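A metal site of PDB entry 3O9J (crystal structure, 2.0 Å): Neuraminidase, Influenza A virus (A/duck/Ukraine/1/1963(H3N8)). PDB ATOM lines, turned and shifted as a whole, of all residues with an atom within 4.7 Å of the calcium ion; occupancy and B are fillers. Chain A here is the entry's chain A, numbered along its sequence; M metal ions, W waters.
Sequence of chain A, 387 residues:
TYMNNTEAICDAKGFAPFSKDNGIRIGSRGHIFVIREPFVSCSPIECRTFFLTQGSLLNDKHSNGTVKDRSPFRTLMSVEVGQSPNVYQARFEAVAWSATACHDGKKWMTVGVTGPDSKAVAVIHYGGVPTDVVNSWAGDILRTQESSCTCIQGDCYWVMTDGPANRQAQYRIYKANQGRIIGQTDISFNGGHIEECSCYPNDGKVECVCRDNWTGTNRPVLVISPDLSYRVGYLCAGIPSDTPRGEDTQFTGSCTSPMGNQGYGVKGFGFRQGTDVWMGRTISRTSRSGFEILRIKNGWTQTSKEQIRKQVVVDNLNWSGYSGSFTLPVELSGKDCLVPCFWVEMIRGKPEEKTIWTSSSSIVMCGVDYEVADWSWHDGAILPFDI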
ATOM      1  N   ASP A 212      -4.600  25.737  21.796  1.00  0.00           N
ATOM      2  CA  ASP A 212      -4.408  24.338  22.140  1.00  0.00           C
ATOM      3  C   ASP A 212      -3.116  23.948  21.431  1.00  0.00           C
ATOM      4  O   ASP A 212      -3.032  23.986  20.197  1.00  0.00           O
ATOM      5  CB  ASP A 212      -5.634  23.502  21.695  1.00  0.00           C
ATOM      6  CG  ASP A 212      -5.484  22.018  21.919  1.00  0.00           C
ATOM      7  OD1 ASP A 212      -6.504  21.327  22.257  1.00  0.00           O
ATOM      8  OD2 ASP A 212      -4.368  21.473  21.699  1.00  0.00           O
ATOM      9  N   ASN A 213      -2.111  23.560  22.207  1.00  0.00           N
ATOM     10  CA  ASN A 213      -0.817  23.226  21.614  1.00  0.00           C
ATOM     11  C   ASN A 213      -0.539  21.715  21.360  1.00  0.00           C
ATOM     12  O   ASN A 213       0.613  21.317  20.870  1.00  0.00           O
ATOM     13  CB  ASN A 213       0.304  23.823  22.473  1.00  0.00           C
ATOM     14  CG  ASN A 213       1.540  24.148  21.665  1.00  0.00           C
ATOM     15  OD1 ASN A 213       1.497  24.925  20.696  1.00  0.00           O
ATOM     16  ND2 ASN A 213       2.679  23.598  22.090  1.00  0.00           N
ATOM     17  N   GLY A 216      -5.210  20.332  18.724  1.00  0.00           N
ATOM     18  CA  GLY A 216      -6.296  21.125  18.214  1.00  0.00           C
ATOM     19  C   GLY A 216      -5.862  22.190  17.269  1.00  0.00           C
ATOM     20  O   GLY A 216      -4.989  22.999  17.586  1.00  0.00           O
ATOM     21  N   THR A 217      -6.515  22.235  16.106  1.00  0.00           N
ATOM     22  CA  THR A 217      -6.371  23.385  15.220  1.00  0.00           C
ATOM     23  C   THR A 217      -7.582  24.311  15.350  1.00  0.00           C
ATOM     24  O   THR A 217      -7.561  25.400  14.748  1.00  0.00           O
ATOM     25  CB  THR A 217      -6.140  22.974  13.777  1.00  0.00           C
ATOM     26  OG1 THR A 217      -7.295  22.306  13.275  1.00  0.00           O
ATOM     27  CG2 THR A 217      -4.941  22.010  13.684  1.00  0.00           C
ATOM     28  N   ASP A 242      -6.046  28.184  14.347  1.00  0.00           N
ATOM     29  CA  ASP A 242      -4.660  28.010  14.811  1.00  0.00           C
ATOM     30  C   ASP A 242      -3.699  27.995  13.629  1.00  0.00           C
ATOM     31  O   ASP A 242      -4.082  28.052  12.439  1.00  0.00           O
ATOM     32  CB  ASP A 242      -4.484  26.718  15.658  1.00  0.00           C
ATOM     33  CG  ASP A 242      -3.478  26.885  16.769  1.00  0.00           C
ATOM     34  OD1 ASP A 242      -3.407  26.053  17.700  1.00  0.00           O
ATOM     35  OD2 ASP A 242      -2.803  27.927  16.791  1.00  0.00           O
ATOM     36  N   GLY A 263      -0.041  19.125  16.135  1.00  0.00           N
ATOM     37  CA  GLY A 263       0.507  19.718  17.329  1.00  0.00           C
ATOM     38  C   GLY A 263       0.787  21.198  17.054  1.00  0.00           C
ATOM     39  O   GLY A 263       0.437  21.752  15.975  1.00  0.00           O
ATOM     40  N   TYR A 264       1.420  21.838  18.041  1.00  0.00           N
ATOM     41  CA  TYR A 264       1.890  23.226  17.963  1.00  0.00           C
ATOM     42  C   TYR A 264       0.749  24.267  17.903  1.00  0.00           C
ATOM     43  O   TYR A 264      -0.362  23.957  18.208  1.00  0.00           O
ATOM     44  CB  TYR A 264       2.942  23.411  16.855  1.00  0.00           C
ATOM     45  CG  TYR A 264       3.878  24.612  17.043  1.00  0.00           C
ATOM     46  CD1 TYR A 264       4.696  24.722  18.175  1.00  0.00           C
ATOM     47  CD2 TYR A 264       3.962  25.628  16.072  1.00  0.00           C
ATOM     48  CE1 TYR A 264       5.566  25.817  18.326  1.00  0.00           C
ATOM     49  CE2 TYR A 264       4.834  26.707  16.216  1.00  0.00           C
ATOM     50  CZ  TYR A 264       5.640  26.791  17.345  1.00  0.00           C
ATOM     51  OH  TYR A 264       6.497  27.848  17.533  1.00  0.00           O
ATOM     52  N   GLY A 265       1.041  25.508  17.554  1.00  0.00           N
ATOM     53  CA  GLY A 265       0.061  26.568  17.788  1.00  0.00           C
ATOM     54  C   GLY A 265       0.648  27.957  17.640  1.00  0.00           C
ATOM     55  O   GLY A 265       1.864  28.124  17.356  1.00  0.00           O
HETATM   56 CA    CA M   1      -2.603  23.621  17.756  1.00  0.00          CA
HETATM   57  O   HOH W   1      -1.998  21.457  18.653  1.00  0.00           O
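The backbone NH (N) of Gly 265 is in hydrogen-bond range of the side-chain amide oxygen (OD1) of Asn 213 (3.2 Å). The backbone NH (N) of Asp 242 is in hydrogen-bond range of the backbone carbonyl oxygen (O) of Thr 217, 3.2 Å away. The backbone NH (N) of Tyr 264 is in hydrogen-bond range of the backbone carbonyl oxygen (O) of Asn 213 (3.0 Å). The side-chain carboxylate (OD2) of Asp 212 sits at hydrogen-bond distance from the backbone NH (N) of Gly 216, at 3.3 Å.
Merely in contact with the calcium ion: Gly 263 and Gly 265. Within 4 Å of the calcium ion: Asp 212, Gly 216, Asp 242, Gly 263, Tyr 264 and Gly 265. The nearest printed residue that does not touch the calcium ion is Asn 213 (4.3 Å).
The calcium ion is bound by O of Tyr 264. Water W1 binds the calcium ion (2.4 Å). The calcium ion is bound by the backbone carbonyl oxygen (O) of Gly 216. O of Asp 212 binds the calcium ion, at 2.5 Å. The calcium ion is bound by OD1 of Asp 242 (2.6 Å). The calcium ion has five donor atoms within binding distance.
Water W1 lies within hydrogen-bond range of the backbone NH (N) of Gly 216 (3.4 Å), the backbone carbonyl oxygen (O) of Asn 213 (3.4 Å) and the backbone NH (N) of Tyr 264 (3.5 Å).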
